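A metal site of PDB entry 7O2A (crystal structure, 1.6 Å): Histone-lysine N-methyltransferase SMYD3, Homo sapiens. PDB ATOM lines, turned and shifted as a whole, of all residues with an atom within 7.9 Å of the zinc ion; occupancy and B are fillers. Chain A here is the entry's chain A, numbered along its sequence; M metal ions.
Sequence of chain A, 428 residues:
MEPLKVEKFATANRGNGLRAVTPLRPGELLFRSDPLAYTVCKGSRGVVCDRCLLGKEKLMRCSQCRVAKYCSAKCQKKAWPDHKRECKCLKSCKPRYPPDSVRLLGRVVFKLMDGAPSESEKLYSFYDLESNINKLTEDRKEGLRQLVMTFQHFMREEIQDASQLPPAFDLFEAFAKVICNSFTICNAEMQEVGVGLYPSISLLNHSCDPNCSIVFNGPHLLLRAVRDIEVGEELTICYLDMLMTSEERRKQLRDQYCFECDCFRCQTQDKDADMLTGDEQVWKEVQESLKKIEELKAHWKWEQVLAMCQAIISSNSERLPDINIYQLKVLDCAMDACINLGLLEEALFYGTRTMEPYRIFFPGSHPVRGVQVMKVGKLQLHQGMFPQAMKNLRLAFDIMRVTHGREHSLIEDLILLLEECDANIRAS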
ATOM      1  N   ASP A  50     -15.169  28.309  28.524  1.00  0.00           N
ATOM      2  CA  ASP A  50     -16.280  27.387  28.859  1.00  0.00           C
ATOM      3  C   ASP A  50     -16.063  26.567  30.085  1.00  0.00           C
ATOM      4  O   ASP A  50     -17.030  26.338  30.852  1.00  0.00           O
ATOM      5  CB  ASP A  50     -16.468  26.390  27.731  1.00  0.00           C
ATOM      6  CG  ASP A  50     -17.528  26.811  26.726  1.00  0.00           C
ATOM      7  OD1 ASP A  50     -17.530  27.952  26.214  1.00  0.00           O
ATOM      8  OD2 ASP A  50     -18.404  25.969  26.458  1.00  0.00           O
ATOM      9  N   ARG A  61     -11.301  28.023  20.070  1.00  0.00           N
ATOM     10  CA  ARG A  61     -12.518  27.283  19.833  1.00  0.00           C
ATOM     11  C   ARG A  61     -12.416  25.804  19.614  1.00  0.00           C
ATOM     12  O   ARG A  61     -11.430  25.304  19.105  1.00  0.00           O
ATOM     13  CB  ARG A  61     -13.263  27.871  18.687  1.00  0.00           C
ATOM     14  CG  ARG A  61     -12.561  27.776  17.370  1.00  0.00           C
ATOM     15  CD  ARG A  61     -13.230  28.715  16.383  1.00  0.00           C
ATOM     16  NE  ARG A  61     -12.486  28.572  15.138  1.00  0.00           N
ATOM     17  CZ  ARG A  61     -12.861  29.055  13.954  1.00  0.00           C
ATOM     18  NH1 ARG A  61     -14.009  29.678  13.826  1.00  0.00           N
ATOM     19  NH2 ARG A  61     -12.096  28.893  12.890  1.00  0.00           N
ATOM     20  N   CYS A  62     -13.468  25.100  19.994  1.00  0.00           N
ATOM     21  CA  CYS A  62     -13.662  23.701  19.625  1.00  0.00           C
ATOM     22  C   CYS A  62     -13.725  23.665  18.148  1.00  0.00           C
ATOM     23  O   CYS A  62     -14.503  24.381  17.548  1.00  0.00           O
ATOM     24  CB  CYS A  62     -14.982  23.102  20.141  1.00  0.00           C
ATOM     25  SG  CYS A  62     -15.306  21.345  19.755  1.00  0.00           S
ATOM     26  N   SER A  63     -12.909  22.813  17.564  1.00  0.00           N
ATOM     27  CA  SER A  63     -12.917  22.729  16.106  1.00  0.00           C
ATOM     28  C   SER A  63     -14.234  22.199  15.501  1.00  0.00           C
ATOM     29  O   SER A  63     -14.649  22.668  14.477  1.00  0.00           O
ATOM     30  CB  SER A  63     -11.731  21.910  15.598  1.00  0.00           C
ATOM     31  OG  SER A  63     -11.801  21.845  14.185  1.00  0.00           O
ATOM     32  N   GLN A  64     -14.824  21.194  16.154  1.00  0.00           N
ATOM     33  CA  GLN A  64     -16.025  20.483  15.657  1.00  0.00           C
ATOM     34  C   GLN A  64     -17.199  21.446  15.677  1.00  0.00           C
ATOM     35  O   GLN A  64     -17.762  21.763  14.624  1.00  0.00           O
ATOM     36  CB  GLN A  64     -16.289  19.181  16.400  1.00  0.00           C
ATOM     37  CG  GLN A  64     -15.174  18.131  16.149  1.00  0.00           C
ATOM     38  CD  GLN A  64     -13.934  18.278  17.065  1.00  0.00           C
ATOM     39  OE1 GLN A  64     -12.899  18.844  16.690  1.00  0.00           O
ATOM     40  NE2 GLN A  64     -14.060  17.769  18.282  1.00  0.00           N
ATOM     41  N   CYS A  65     -17.562  21.992  16.847  1.00  0.00           N
ATOM     42  CA  CYS A  65     -18.743  22.907  16.881  1.00  0.00           C
ATOM     43  C   CYS A  65     -18.431  24.375  16.651  1.00  0.00           C
ATOM     44  O   CYS A  65     -19.307  25.095  16.248  1.00  0.00           O
ATOM     45  CB  CYS A  65     -19.496  22.778  18.241  1.00  0.00           C
ATOM     46  SG  CYS A  65     -18.534  23.209  19.690  1.00  0.00           S
ATOM     47  N   ARG A  66     -17.210  24.833  16.978  1.00  0.00           N
ATOM     48  CA  ARG A  66     -16.873  26.252  17.000  1.00  0.00           C
ATOM     49  C   ARG A  66     -17.752  27.155  17.909  1.00  0.00           C
ATOM     50  O   ARG A  66     -17.776  28.376  17.731  1.00  0.00           O
ATOM     51  CB  ARG A  66     -16.832  26.776  15.572  1.00  0.00           C
ATOM     52  CG  ARG A  66     -15.726  26.088  14.803  1.00  0.00           C
ATOM     53  CD  ARG A  66     -15.686  26.623  13.394  1.00  0.00           C
ATOM     54  NE  ARG A  66     -14.470  26.215  12.742  1.00  0.00           N
ATOM     55  CZ  ARG A  66     -14.150  26.550  11.494  1.00  0.00           C
ATOM     56  NH1 ARG A  66     -14.975  27.337  10.777  1.00  0.00           N
ATOM     57  NH2 ARG A  66     -12.990  26.110  10.967  1.00  0.00           N
ATOM     58  N   VAL A  67     -18.386  26.566  18.930  1.00  0.00           N
ATOM     59  CA  VAL A  67     -19.177  27.364  19.885  1.00  0.00           C
ATOM     60  C   VAL A  67     -18.490  27.426  21.284  1.00  0.00           C
ATOM     61  O   VAL A  67     -18.328  28.495  21.883  1.00  0.00           O
ATOM     62  CB  VAL A  67     -20.602  26.764  19.952  1.00  0.00           C
ATOM     63  CG1 VAL A  67     -21.418  27.414  21.087  1.00  0.00           C
ATOM     64  CG2 VAL A  67     -21.293  26.850  18.603  1.00  0.00           C
ATOM     65  N   ALA A  68     -18.083  26.241  21.740  1.00  0.00           N
ATOM     66  CA  ALA A  68     -17.305  26.106  22.974  1.00  0.00           C
ATOM     67  C   ALA A  68     -15.937  26.738  22.739  1.00  0.00           C
ATOM     68  O   ALA A  68     -15.350  26.516  21.656  1.00  0.00           O
ATOM     69  CB  ALA A  68     -17.221  24.660  23.365  1.00  0.00           C
ATOM     70  N   LYS A  69     -15.466  27.572  23.688  1.00  0.00           N
ATOM     71  CA  LYS A  69     -14.152  28.192  23.607  1.00  0.00           C
ATOM     72  C   LYS A  69     -13.431  28.076  24.922  1.00  0.00           C
ATOM     73  O   LYS A  69     -14.079  27.987  25.981  1.00  0.00           O
ATOM     74  CB  LYS A  69     -14.211  29.653  23.175  1.00  0.00           C
ATOM     75  CG  LYS A  69     -14.993  29.788  21.904  1.00  0.00           C
ATOM     76  CD  LYS A  69     -14.976  31.154  21.275  1.00  0.00           C
ATOM     77  CE  LYS A  69     -15.631  31.093  19.891  1.00  0.00           C
ATOM     78  NZ  LYS A  69     -16.285  32.372  19.514  1.00  0.00           N
ATOM     79  N   TYR A  70     -12.110  28.005  24.879  1.00  0.00           N
ATOM     80  CA  TYR A  70     -11.361  27.600  26.043  1.00  0.00           C
ATOM     81  C   TYR A  70     -10.118  28.414  26.208  1.00  0.00           C
ATOM     82  O   TYR A  70      -9.556  28.999  25.246  1.00  0.00           O
ATOM     83  CB  TYR A  70     -10.926  26.150  25.906  1.00  0.00           C
ATOM     84  CG  TYR A  70     -12.102  25.237  25.751  1.00  0.00           C
ATOM     85  CD1 TYR A  70     -12.844  24.856  26.867  1.00  0.00           C
ATOM     86  CD2 TYR A  70     -12.496  24.770  24.486  1.00  0.00           C
ATOM     87  CE1 TYR A  70     -13.936  23.992  26.736  1.00  0.00           C
ATOM     88  CE2 TYR A  70     -13.571  23.896  24.366  1.00  0.00           C
ATOM     89  CZ  TYR A  70     -14.306  23.559  25.482  1.00  0.00           C
ATOM     90  OH  TYR A  70     -15.364  22.661  25.414  1.00  0.00           O
ATOM     91  N   GLN A  76      -9.704  22.732  27.344  1.00  0.00           N
ATOM     92  CA  GLN A  76     -10.475  22.131  26.224  1.00  0.00           C
ATOM     93  C   GLN A  76     -10.520  20.610  26.381  1.00  0.00           C
ATOM     94  O   GLN A  76     -11.564  19.977  26.201  1.00  0.00           O
ATOM     95  CB  GLN A  76      -9.827  22.543  24.887  1.00  0.00           C
ATOM     96  CG  GLN A  76     -10.565  21.958  23.742  1.00  0.00           C
ATOM     97  CD  GLN A  76     -10.208  22.533  22.404  1.00  0.00           C
ATOM     98  OE1 GLN A  76      -9.471  23.540  22.288  1.00  0.00           O
ATOM     99  NE2 GLN A  76     -10.746  21.942  21.382  1.00  0.00           N
ATOM    100  N   TRP A  80     -13.810  17.950  27.474  1.00  0.00           N
ATOM    101  CA  TRP A  80     -14.343  17.172  26.357  1.00  0.00           C
ATOM    102  C   TRP A  80     -15.399  16.153  26.800  1.00  0.00           C
ATOM    103  O   TRP A  80     -16.437  16.064  26.127  1.00  0.00           O
ATOM    104  CB  TRP A  80     -13.243  16.531  25.522  1.00  0.00           C
ATOM    105  CG  TRP A  80     -13.736  15.621  24.472  1.00  0.00           C
ATOM    106  CD1 TRP A  80     -13.621  14.256  24.487  1.00  0.00           C
ATOM    107  CD2 TRP A  80     -14.434  15.966  23.273  1.00  0.00           C
ATOM    108  NE1 TRP A  80     -14.251  13.733  23.385  1.00  0.00           N
ATOM    109  CE2 TRP A  80     -14.731  14.756  22.612  1.00  0.00           C
ATOM    110  CE3 TRP A  80     -14.874  17.165  22.702  1.00  0.00           C
ATOM    111  CZ2 TRP A  80     -15.398  14.713  21.391  1.00  0.00           C
ATOM    112  CZ3 TRP A  80     -15.500  17.129  21.498  1.00  0.00           C
ATOM    113  CH2 TRP A  80     -15.790  15.924  20.839  1.00  0.00           C
ATOM    114  N   HIS A  83     -18.565  17.861  27.160  1.00  0.00           N
ATOM    115  CA  HIS A  83     -18.956  18.633  25.970  1.00  0.00           C
ATOM    116  C   HIS A  83     -19.262  17.754  24.721  1.00  0.00           C
ATOM    117  O   HIS A  83     -19.878  18.226  23.796  1.00  0.00           O
ATOM    118  CB  HIS A  83     -17.812  19.535  25.659  1.00  0.00           C
ATOM    119  CG  HIS A  83     -17.970  20.273  24.373  1.00  0.00           C
ATOM    120  ND1 HIS A  83     -19.026  21.134  24.148  1.00  0.00           N
ATOM    121  CD2 HIS A  83     -17.241  20.256  23.240  1.00  0.00           C
ATOM    122  CE1 HIS A  83     -18.956  21.619  22.923  1.00  0.00           C
ATOM    123  NE2 HIS A  83     -17.879  21.102  22.347  1.00  0.00           N
ATOM    124  N   LYS A  84     -18.807  16.494  24.724  1.00  0.00           N
ATOM    125  CA  LYS A  84     -18.818  15.570  23.576  1.00  0.00           C
ATOM    126  C   LYS A  84     -20.208  15.494  22.925  1.00  0.00           C
ATOM    127  O   LYS A  84     -20.356  15.598  21.706  1.00  0.00           O
ATOM    128  CB  LYS A  84     -18.336  14.178  24.073  1.00  0.00           C
ATOM    129  CG  LYS A  84     -18.528  13.029  23.103  1.00  0.00           C
ATOM    130  CD  LYS A  84     -17.574  11.878  23.311  1.00  0.00           C
ATOM    131  CE  LYS A  84     -17.709  11.230  24.667  1.00  0.00           C
ATOM    132  NZ  LYS A  84     -18.780  10.174  24.649  1.00  0.00           N
ATOM    133  N   ARG A  85     -21.232  15.288  23.760  1.00  0.00           N
ATOM    134  CA  ARG A  85     -22.552  15.026  23.210  1.00  0.00           C
ATOM    135  C   ARG A  85     -23.203  16.330  22.849  1.00  0.00           C
ATOM    136  O   ARG A  85     -23.890  16.384  21.841  1.00  0.00           O
ATOM    137  CB  ARG A  85     -23.405  14.221  24.166  1.00  0.00           C
ATOM    138  CG  ARG A  85     -22.805  12.860  24.440  1.00  0.00           C
ATOM    139  CD  ARG A  85     -23.655  11.940  25.252  1.00  0.00           C
ATOM    140  NE  ARG A  85     -24.905  11.680  24.560  1.00  0.00           N
ATOM    141  CZ  ARG A  85     -25.960  11.076  25.078  1.00  0.00           C
ATOM    142  NH1 ARG A  85     -25.945  10.628  26.307  1.00  0.00           N
ATOM    143  NH2 ARG A  85     -27.066  10.958  24.358  1.00  0.00           N
ATOM    144  N   GLU A  86     -22.984  17.409  23.600  1.00  0.00           N
ATOM    145  CA  GLU A  86     -23.626  18.646  23.186  1.00  0.00           C
ATOM    146  C   GLU A  86     -22.965  19.190  21.925  1.00  0.00           C
ATOM    147  O   GLU A  86     -23.537  19.998  21.183  1.00  0.00           O
ATOM    148  CB  GLU A  86     -23.664  19.710  24.331  1.00  0.00           C
ATOM    149  CG  GLU A  86     -22.320  20.313  24.655  1.00  0.00           C
ATOM    150  CD  GLU A  86     -22.282  21.578  25.508  1.00  0.00           C
ATOM    151  OE1 GLU A  86     -23.316  22.025  26.060  1.00  0.00           O
ATOM    152  OE2 GLU A  86     -21.149  22.091  25.669  1.00  0.00           O
ATOM    153  N   CYS A  87     -21.701  18.830  21.723  1.00  0.00           N
ATOM    154  CA  CYS A  87     -20.935  19.383  20.569  1.00  0.00           C
ATOM    155  C   CYS A  87     -21.683  19.178  19.225  1.00  0.00           C
ATOM    156  O   CYS A  87     -21.854  20.099  18.452  1.00  0.00           O
ATOM    157  CB  CYS A  87     -19.568  18.677  20.494  1.00  0.00           C
ATOM    158  SG  CYS A  87     -18.483  19.387  19.264  1.00  0.00           S
ATOM    159  N   LYS A  88     -22.152  17.959  19.056  1.00  0.00           N
ATOM    160  CA  LYS A  88     -22.904  17.553  17.853  1.00  0.00           C
ATOM    161  C   LYS A  88     -24.183  18.362  17.723  1.00  0.00           C
ATOM    162  O   LYS A  88     -24.483  18.922  16.677  1.00  0.00           O
ATOM    163  CB  LYS A  88     -23.182  16.055  17.923  1.00  0.00           C
ATOM    164  CG  LYS A  88     -21.906  15.220  18.036  1.00  0.00           C
ATOM    165  CD  LYS A  88     -21.905  14.032  17.104  1.00  0.00           C
ATOM    166  CE  LYS A  88     -20.599  13.293  17.280  1.00  0.00           C
ATOM    167  NZ  LYS A  88     -20.284  12.430  16.105  1.00  0.00           N
ATOM    168  N   LEU A  90     -24.859  21.391  19.108  1.00  0.00           N
ATOM    169  CA  LEU A  90     -24.541  22.796  18.834  1.00  0.00           C
ATOM    170  C   LEU A  90     -24.067  22.986  17.362  1.00  0.00           C
ATOM    171  O   LEU A  90     -24.302  24.026  16.773  1.00  0.00           O
ATOM    172  CB  LEU A  90     -23.453  23.311  19.765  1.00  0.00           C
ATOM    173  CG  LEU A  90     -23.717  23.461  21.277  1.00  0.00           C
ATOM    174  CD1 LEU A  90     -22.391  23.500  22.050  1.00  0.00           C
ATOM    175  CD2 LEU A  90     -24.522  24.702  21.599  1.00  0.00           C
ATOM    176  N   LYS A  91     -23.393  21.972  16.813  1.00  0.00           N
ATOM    177  CA  LYS A  91     -22.943  22.001  15.399  1.00  0.00           C
ATOM    178  C   LYS A  91     -24.231  21.931  14.562  1.00  0.00           C
ATOM    179  O   LYS A  91     -24.633  22.934  13.939  1.00  0.00           O
ATOM    180  CB  LYS A  91     -21.980  20.836  15.080  1.00  0.00           C
ATOM    181  CG  LYS A  91     -20.946  21.161  14.009  1.00  0.00           C
ATOM    182  CD  LYS A  91     -21.410  20.844  12.587  1.00  0.00           C
ATOM    183  CE  LYS A  91     -20.818  21.800  11.543  1.00  0.00           C
ATOM    184  NZ  LYS A  91     -19.318  21.902  11.596  1.00  0.00           N
ATOM    185  N   ARG A 103     -29.294  24.682  27.128  1.00  0.00           N
ATOM    186  CA  ARG A 103     -27.932  24.135  27.123  1.00  0.00           C
ATOM    187  C   ARG A 103     -27.670  23.469  28.492  1.00  0.00           C
ATOM    188  O   ARG A 103     -27.093  22.348  28.565  1.00  0.00           O
ATOM    189  CB  ARG A 103     -26.948  25.212  26.753  1.00  0.00           C
ATOM    190  CG  ARG A 103     -25.535  24.646  26.592  1.00  0.00           C
ATOM    191  CD  ARG A 103     -24.572  25.605  25.926  1.00  0.00           C
ATOM    192  NE  ARG A 103     -23.220  25.010  25.793  1.00  0.00           N
ATOM    193  CZ  ARG A 103     -22.112  25.704  25.514  1.00  0.00           C
ATOM    194  NH1 ARG A 103     -22.139  27.033  25.344  1.00  0.00           N
ATOM    195  NH2 ARG A 103     -20.934  25.058  25.372  1.00  0.00           N
HETATM  196 ZN    ZN M   1     -17.505  21.261  20.230  1.00  0.00          ZN
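A ring nitrogen (ND1) of His 83 is in hydrogen-bond range of the side-chain carboxylate (OE2) of Glu 86 (2.8 Å). N of Gln 64 lies close to SG of Cys 62. The backbone NH (N) of Cys 62 lies within hydrogen-bond range of the backbone carbonyl oxygen (O) of Ala 68 (2.9 Å). SG of Cys 65 lies close to N of Ala 68, at 3.7 Å. The backbone NH (N) of Val 67 sits close to the side-chain sulfur (SG) of Cys 65, 3.4 Å away.
Within 4 Å of the zinc ion: Cys 62, Cys 65, His 83 and Cys 87.
The zinc ion is bound by a ring nitrogen (NE2) of His 83 (2.2 Å), the side-chain sulfur of Cys 62 (2.3 Å), the side-chain sulfur of Cys 65 (2.3 Å) and the side-chain sulfur of Cys 87 (2.3 Å). The zinc ion has four donor atoms within binding distance.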
